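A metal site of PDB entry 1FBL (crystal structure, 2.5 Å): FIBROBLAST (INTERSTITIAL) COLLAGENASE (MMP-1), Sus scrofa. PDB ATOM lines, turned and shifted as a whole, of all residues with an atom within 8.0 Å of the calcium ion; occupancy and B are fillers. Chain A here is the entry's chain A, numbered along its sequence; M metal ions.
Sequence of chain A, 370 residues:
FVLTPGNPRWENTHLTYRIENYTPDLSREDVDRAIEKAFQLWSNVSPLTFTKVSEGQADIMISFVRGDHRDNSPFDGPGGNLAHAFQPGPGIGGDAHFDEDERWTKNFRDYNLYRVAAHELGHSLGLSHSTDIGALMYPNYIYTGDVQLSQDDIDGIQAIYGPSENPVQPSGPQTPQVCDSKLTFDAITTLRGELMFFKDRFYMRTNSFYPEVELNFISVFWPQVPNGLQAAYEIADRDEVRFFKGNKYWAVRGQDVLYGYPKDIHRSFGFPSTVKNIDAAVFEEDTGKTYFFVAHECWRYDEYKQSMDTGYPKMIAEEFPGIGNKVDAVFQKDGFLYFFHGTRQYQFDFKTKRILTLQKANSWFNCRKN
O of Asp 279 binds the calcium ion, at 2.2 Å. The calcium ion is bound by O of Gln 230, at 2.4 Å. The calcium ion is bound by the backbone carbonyl oxygen (O) of Asp 186 (2.5 Å). The calcium ion is bound by O of Asp 328, 2.5 Å away.
Of the 23 residues printed, 4 come within 4 Å of the calcium ion.
N of Asp 279 sits at hydrogen-bond distance from O of Phe 293, 2.8 Å away. N of Asp 186 lies within hydrogen-bond range of O of Phe 198, at 3.1 Å. N of Asp 328 is in hydrogen-bond range of O of Phe 340 (2.8 Å). The side-chain amino group (NZ) of Lys 326 is in salt-bridge range of the side-chain carboxylate (OD1) of Asp 328, 3.7 Å away. The backbone NH (N) of Gln 230 lies within hydrogen-bond range of the backbone carbonyl oxygen (O) of Phe 244, 2.8 Å away.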
ATOM      1  N   PHE A 185     -14.333 -15.285   5.474  1.00  0.00           N
ATOM      2  CA  PHE A 185     -13.703 -16.557   5.726  1.00  0.00           C
ATOM      3  C   PHE A 185     -13.797 -17.544   4.561  1.00  0.00           C
ATOM      4  O   PHE A 185     -14.708 -17.457   3.736  1.00  0.00           O
ATOM      5  CB  PHE A 185     -14.282 -17.173   7.013  1.00  0.00           C
ATOM      6  CG  PHE A 185     -14.055 -16.316   8.235  1.00  0.00           C
ATOM      7  CD1 PHE A 185     -12.785 -16.217   8.788  1.00  0.00           C
ATOM      8  CD2 PHE A 185     -15.045 -15.498   8.740  1.00  0.00           C
ATOM      9  CE1 PHE A 185     -12.531 -15.312   9.806  1.00  0.00           C
ATOM     10  CE2 PHE A 185     -14.782 -14.598   9.758  1.00  0.00           C
ATOM     11  CZ  PHE A 185     -13.526 -14.508  10.277  1.00  0.00           C
ATOM     12  N   ASP A 186     -12.802 -18.449   4.492  1.00  0.00           N
ATOM     13  CA  ASP A 186     -12.709 -19.552   3.509  1.00  0.00           C
ATOM     14  C   ASP A 186     -13.504 -20.765   4.019  1.00  0.00           C
ATOM     15  O   ASP A 186     -14.319 -21.346   3.265  1.00  0.00           O
ATOM     16  CB  ASP A 186     -11.252 -20.025   3.325  1.00  0.00           C
ATOM     17  CG  ASP A 186     -10.387 -19.067   2.510  1.00  0.00           C
ATOM     18  OD1 ASP A 186     -10.815 -17.964   2.148  1.00  0.00           O
ATOM     19  OD2 ASP A 186      -9.245 -19.445   2.231  1.00  0.00           O
ATOM     20  N   ALA A 187     -13.221 -21.148   5.268  1.00  0.00           N
ATOM     21  CA  ALA A 187     -13.875 -22.261   5.948  1.00  0.00           C
ATOM     22  C   ALA A 187     -13.810 -22.084   7.469  1.00  0.00           C
ATOM     23  O   ALA A 187     -13.056 -21.280   7.978  1.00  0.00           O
ATOM     24  CB  ALA A 187     -13.236 -23.537   5.559  1.00  0.00           C
ATOM     25  N   ILE A 188     -14.613 -22.842   8.192  1.00  0.00           N
ATOM     26  CA  ILE A 188     -14.623 -22.778   9.643  1.00  0.00           C
ATOM     27  C   ILE A 188     -15.107 -24.105  10.187  1.00  0.00           C
ATOM     28  O   ILE A 188     -16.146 -24.595   9.769  1.00  0.00           O
ATOM     29  CB  ILE A 188     -15.607 -21.724  10.166  1.00  0.00           C
ATOM     30  CG1 ILE A 188     -15.228 -20.326   9.698  1.00  0.00           C
ATOM     31  CG2 ILE A 188     -15.659 -21.773  11.706  1.00  0.00           C
ATOM     32  CD1 ILE A 188     -16.237 -19.314  10.115  1.00  0.00           C
ATOM     33  N   PHE A 198     -10.547 -20.482   9.047  1.00  0.00           N
ATOM     34  CA  PHE A 198      -9.506 -20.622   8.046  1.00  0.00           C
ATOM     35  C   PHE A 198      -9.535 -19.484   7.036  1.00  0.00           C
ATOM     36  O   PHE A 198     -10.596 -19.012   6.660  1.00  0.00           O
ATOM     37  CB  PHE A 198      -9.642 -22.006   7.350  1.00  0.00           C
ATOM     38  CG  PHE A 198      -9.403 -23.206   8.278  1.00  0.00           C
ATOM     39  CD1 PHE A 198      -8.093 -23.613   8.612  1.00  0.00           C
ATOM     40  CD2 PHE A 198     -10.481 -23.932   8.823  1.00  0.00           C
ATOM     41  CE1 PHE A 198      -7.876 -24.710   9.471  1.00  0.00           C
ATOM     42  CE2 PHE A 198     -10.263 -25.029   9.682  1.00  0.00           C
ATOM     43  CZ  PHE A 198      -8.971 -25.406  10.004  1.00  0.00           C
ATOM     44  N   GLY A 228      -5.602 -22.275   1.239  1.00  0.00           N
ATOM     45  CA  GLY A 228      -6.783 -22.079   0.416  1.00  0.00           C
ATOM     46  C   GLY A 228      -7.863 -23.140   0.645  1.00  0.00           C
ATOM     47  O   GLY A 228      -8.495 -23.630  -0.305  1.00  0.00           O
ATOM     48  N   LEU A 229      -8.086 -23.501   1.906  1.00  0.00           N
ATOM     49  CA  LEU A 229      -9.107 -24.485   2.176  1.00  0.00           C
ATOM     50  C   LEU A 229     -10.431 -23.932   1.654  1.00  0.00           C
ATOM     51  O   LEU A 229     -10.606 -22.709   1.599  1.00  0.00           O
ATOM     52  CB  LEU A 229      -9.176 -24.731   3.668  1.00  0.00           C
ATOM     53  CG  LEU A 229      -7.895 -25.319   4.227  1.00  0.00           C
ATOM     54  CD1 LEU A 229      -8.112 -25.644   5.668  1.00  0.00           C
ATOM     55  CD2 LEU A 229      -7.537 -26.584   3.427  1.00  0.00           C
ATOM     56  N   GLN A 230     -11.360 -24.823   1.261  1.00  0.00           N
ATOM     57  CA  GLN A 230     -12.692 -24.413   0.775  1.00  0.00           C
ATOM     58  C   GLN A 230     -13.776 -24.714   1.771  1.00  0.00           C
ATOM     59  O   GLN A 230     -14.784 -23.992   1.826  1.00  0.00           O
ATOM     60  CB  GLN A 230     -13.057 -25.090  -0.550  1.00  0.00           C
ATOM     61  CG  GLN A 230     -12.240 -24.638  -1.761  1.00  0.00           C
ATOM     62  CD  GLN A 230     -12.364 -25.614  -2.906  1.00  0.00           C
ATOM     63  OE1 GLN A 230     -12.189 -25.245  -4.059  1.00  0.00           O
ATOM     64  NE2 GLN A 230     -12.658 -26.885  -2.588  1.00  0.00           N
ATOM     65  N   ALA A 231     -13.626 -25.808   2.487  1.00  0.00           N
ATOM     66  CA  ALA A 231     -14.507 -26.158   3.600  1.00  0.00           C
ATOM     67  C   ALA A 231     -13.728 -27.062   4.569  1.00  0.00           C
ATOM     68  O   ALA A 231     -12.743 -27.679   4.154  1.00  0.00           O
ATOM     69  CB  ALA A 231     -15.753 -26.869   3.088  1.00  0.00           C
ATOM     70  N   ALA A 232     -14.139 -27.104   5.838  1.00  0.00           N
ATOM     71  CA  ALA A 232     -13.489 -27.944   6.869  1.00  0.00           C
ATOM     72  C   ALA A 232     -14.565 -28.341   7.862  1.00  0.00           C
ATOM     73  O   ALA A 232     -15.267 -27.485   8.371  1.00  0.00           O
ATOM     74  CB  ALA A 232     -12.383 -27.171   7.598  1.00  0.00           C
ATOM     75  N   PHE A 244     -11.119 -29.600   2.801  1.00  0.00           N
ATOM     76  CA  PHE A 244     -11.507 -29.775   1.421  1.00  0.00           C
ATOM     77  C   PHE A 244     -10.839 -28.729   0.537  1.00  0.00           C
ATOM     78  O   PHE A 244     -10.840 -27.555   0.868  1.00  0.00           O
ATOM     79  CB  PHE A 244     -13.046 -29.664   1.267  1.00  0.00           C
ATOM     80  CG  PHE A 244     -13.822 -30.832   1.847  1.00  0.00           C
ATOM     81  CD1 PHE A 244     -14.129 -30.900   3.211  1.00  0.00           C
ATOM     82  CD2 PHE A 244     -14.316 -31.832   1.014  1.00  0.00           C
ATOM     83  CE1 PHE A 244     -14.913 -31.936   3.743  1.00  0.00           C
ATOM     84  CE2 PHE A 244     -15.095 -32.880   1.541  1.00  0.00           C
ATOM     85  CZ  PHE A 244     -15.388 -32.921   2.914  1.00  0.00           C
ATOM     86  N   ASN A 277     -15.658 -28.466  -6.883  1.00  0.00           N
ATOM     87  CA  ASN A 277     -15.221 -28.064  -5.534  1.00  0.00           C
ATOM     88  C   ASN A 277     -16.412 -27.724  -4.640  1.00  0.00           C
ATOM     89  O   ASN A 277     -17.498 -27.450  -5.128  1.00  0.00           O
ATOM     90  CB  ASN A 277     -14.232 -26.869  -5.585  1.00  0.00           C
ATOM     91  CG  ASN A 277     -14.830 -25.607  -6.218  1.00  0.00           C
ATOM     92  OD1 ASN A 277     -14.419 -25.206  -7.291  1.00  0.00           O
ATOM     93  ND2 ASN A 277     -15.756 -24.969  -5.529  1.00  0.00           N
ATOM     94  N   ILE A 278     -16.230 -27.786  -3.314  1.00  0.00           N
ATOM     95  CA  ILE A 278     -17.321 -27.422  -2.406  1.00  0.00           C
ATOM     96  C   ILE A 278     -17.137 -26.072  -1.676  1.00  0.00           C
ATOM     97  O   ILE A 278     -16.066 -25.469  -1.714  1.00  0.00           O
ATOM     98  CB  ILE A 278     -17.702 -28.574  -1.396  1.00  0.00           C
ATOM     99  CG1 ILE A 278     -16.641 -28.773  -0.316  1.00  0.00           C
ATOM    100  CG2 ILE A 278     -18.002 -29.865  -2.134  1.00  0.00           C
ATOM    101  CD1 ILE A 278     -17.223 -29.496   0.884  1.00  0.00           C
ATOM    102  N   ASP A 279     -18.202 -25.585  -1.039  1.00  0.00           N
ATOM    103  CA  ASP A 279     -18.169 -24.281  -0.403  1.00  0.00           C
ATOM    104  C   ASP A 279     -18.161 -24.237   1.117  1.00  0.00           C
ATOM    105  O   ASP A 279     -17.631 -23.267   1.702  1.00  0.00           O
ATOM    106  CB  ASP A 279     -19.310 -23.407  -0.914  1.00  0.00           C
ATOM    107  CG  ASP A 279     -19.209 -23.116  -2.381  1.00  0.00           C
ATOM    108  OD1 ASP A 279     -18.107 -23.254  -2.922  1.00  0.00           O
ATOM    109  OD2 ASP A 279     -20.231 -22.755  -2.989  1.00  0.00           O
ATOM    110  N   ALA A 280     -18.758 -25.244   1.745  1.00  0.00           N
ATOM    111  CA  ALA A 280     -18.798 -25.351   3.195  1.00  0.00           C
ATOM    112  C   ALA A 280     -19.325 -26.745   3.552  1.00  0.00           C
ATOM    113  O   ALA A 280     -19.762 -27.462   2.662  1.00  0.00           O
ATOM    114  CB  ALA A 280     -19.711 -24.262   3.752  1.00  0.00           C
ATOM    115  N   ALA A 281     -19.266 -27.145   4.819  1.00  0.00           N
ATOM    116  CA  ALA A 281     -19.828 -28.447   5.216  1.00  0.00           C
ATOM    117  C   ALA A 281     -20.032 -28.516   6.714  1.00  0.00           C
ATOM    118  O   ALA A 281     -19.213 -27.996   7.458  1.00  0.00           O
ATOM    119  CB  ALA A 281     -18.916 -29.568   4.774  1.00  0.00           C
ATOM    120  N   PHE A 293     -22.373 -27.798   1.073  1.00  0.00           N
ATOM    121  CA  PHE A 293     -22.930 -26.667   0.341  1.00  0.00           C
ATOM    122  C   PHE A 293     -22.139 -26.453  -0.945  1.00  0.00           C
ATOM    123  O   PHE A 293     -20.920 -26.323  -0.901  1.00  0.00           O
ATOM    124  CB  PHE A 293     -22.913 -25.405   1.238  1.00  0.00           C
ATOM    125  CG  PHE A 293     -23.799 -25.527   2.459  1.00  0.00           C
ATOM    126  CD1 PHE A 293     -25.163 -25.213   2.390  1.00  0.00           C
ATOM    127  CD2 PHE A 293     -23.273 -25.989   3.665  1.00  0.00           C
ATOM    128  CE1 PHE A 293     -26.001 -25.367   3.500  1.00  0.00           C
ATOM    129  CE2 PHE A 293     -24.102 -26.145   4.790  1.00  0.00           C
ATOM    130  CZ  PHE A 293     -25.466 -25.837   4.693  1.00  0.00           C
ATOM    131  N   LYS A 326     -25.708 -18.710  -1.493  1.00  0.00           N
ATOM    132  CA  LYS A 326     -24.387 -19.295  -1.319  1.00  0.00           C
ATOM    133  C   LYS A 326     -23.948 -19.146   0.102  1.00  0.00           C
ATOM    134  O   LYS A 326     -24.449 -18.286   0.821  1.00  0.00           O
ATOM    135  CB  LYS A 326     -23.356 -18.621  -2.227  1.00  0.00           C
ATOM    136  CG  LYS A 326     -21.967 -19.237  -2.143  1.00  0.00           C
ATOM    137  CD  LYS A 326     -21.206 -19.017  -3.436  1.00  0.00           C
ATOM    138  CE  LYS A 326     -19.726 -19.282  -3.236  1.00  0.00           C
ATOM    139  NZ  LYS A 326     -19.121 -18.290  -2.283  1.00  0.00           N
ATOM    140  N   VAL A 327     -22.994 -19.980   0.496  1.00  0.00           N
ATOM    141  CA  VAL A 327     -22.433 -20.001   1.838  1.00  0.00           C
ATOM    142  C   VAL A 327     -20.894 -19.942   1.763  1.00  0.00           C
ATOM    143  O   VAL A 327     -20.288 -20.490   0.827  1.00  0.00           O
ATOM    144  CB  VAL A 327     -22.871 -21.299   2.598  1.00  0.00           C
ATOM    145  CG1 VAL A 327     -22.545 -21.228   4.102  1.00  0.00           C
ATOM    146  CG2 VAL A 327     -24.367 -21.554   2.393  1.00  0.00           C
ATOM    147  N   ASP A 328     -20.280 -19.224   2.705  1.00  0.00           N
ATOM    148  CA  ASP A 328     -18.833 -19.146   2.802  1.00  0.00           C
ATOM    149  C   ASP A 328     -18.294 -20.245   3.715  1.00  0.00           C
ATOM    150  O   ASP A 328     -17.348 -20.955   3.342  1.00  0.00           O
ATOM    151  CB  ASP A 328     -18.387 -17.770   3.338  1.00  0.00           C
ATOM    152  CG  ASP A 328     -18.213 -16.730   2.248  1.00  0.00           C
ATOM    153  OD1 ASP A 328     -18.684 -16.968   1.127  1.00  0.00           O
ATOM    154  OD2 ASP A 328     -17.614 -15.666   2.502  1.00  0.00           O
ATOM    155  N   ALA A 329     -18.905 -20.406   4.891  1.00  0.00           N
ATOM    156  CA  ALA A 329     -18.482 -21.363   5.918  1.00  0.00           C
ATOM    157  C   ALA A 329     -19.607 -21.543   6.933  1.00  0.00           C
ATOM    158  O   ALA A 329     -20.425 -20.653   7.094  1.00  0.00           O
ATOM    159  CB  ALA A 329     -17.245 -20.846   6.605  1.00  0.00           C
ATOM    160  N   VAL A 330     -19.668 -22.681   7.607  1.00  0.00           N
ATOM    161  CA  VAL A 330     -20.741 -22.967   8.556  1.00  0.00           C
ATOM    162  C   VAL A 330     -20.238 -23.962   9.601  1.00  0.00           C
ATOM    163  O   VAL A 330     -19.340 -24.733   9.321  1.00  0.00           O
ATOM    164  CB  VAL A 330     -21.991 -23.580   7.844  1.00  0.00           C
ATOM    165  CG1 VAL A 330     -21.604 -24.716   6.923  1.00  0.00           C
ATOM    166  CG2 VAL A 330     -23.009 -24.059   8.857  1.00  0.00           C
ATOM    167  N   PHE A 340     -22.195 -18.555   7.285  1.00  0.00           N
ATOM    168  CA  PHE A 340     -21.371 -17.392   6.950  1.00  0.00           C
ATOM    169  C   PHE A 340     -21.500 -16.973   5.523  1.00  0.00           C
ATOM    170  O   PHE A 340     -21.624 -17.802   4.645  1.00  0.00           O
ATOM    171  CB  PHE A 340     -19.870 -17.644   7.262  1.00  0.00           C
ATOM    172  CG  PHE A 340     -19.529 -17.574   8.722  1.00  0.00           C
ATOM    173  CD1 PHE A 340     -19.711 -18.666   9.549  1.00  0.00           C
ATOM    174  CD2 PHE A 340     -19.170 -16.364   9.302  1.00  0.00           C
ATOM    175  CE1 PHE A 340     -19.552 -18.544  10.926  1.00  0.00           C
ATOM    176  CE2 PHE A 340     -19.008 -16.261  10.668  1.00  0.00           C
ATOM    177  CZ  PHE A 340     -19.202 -17.334  11.477  1.00  0.00           C
HETATM  178 CA    CA M   1     -15.930 -21.865   1.472  1.00  0.00          CA
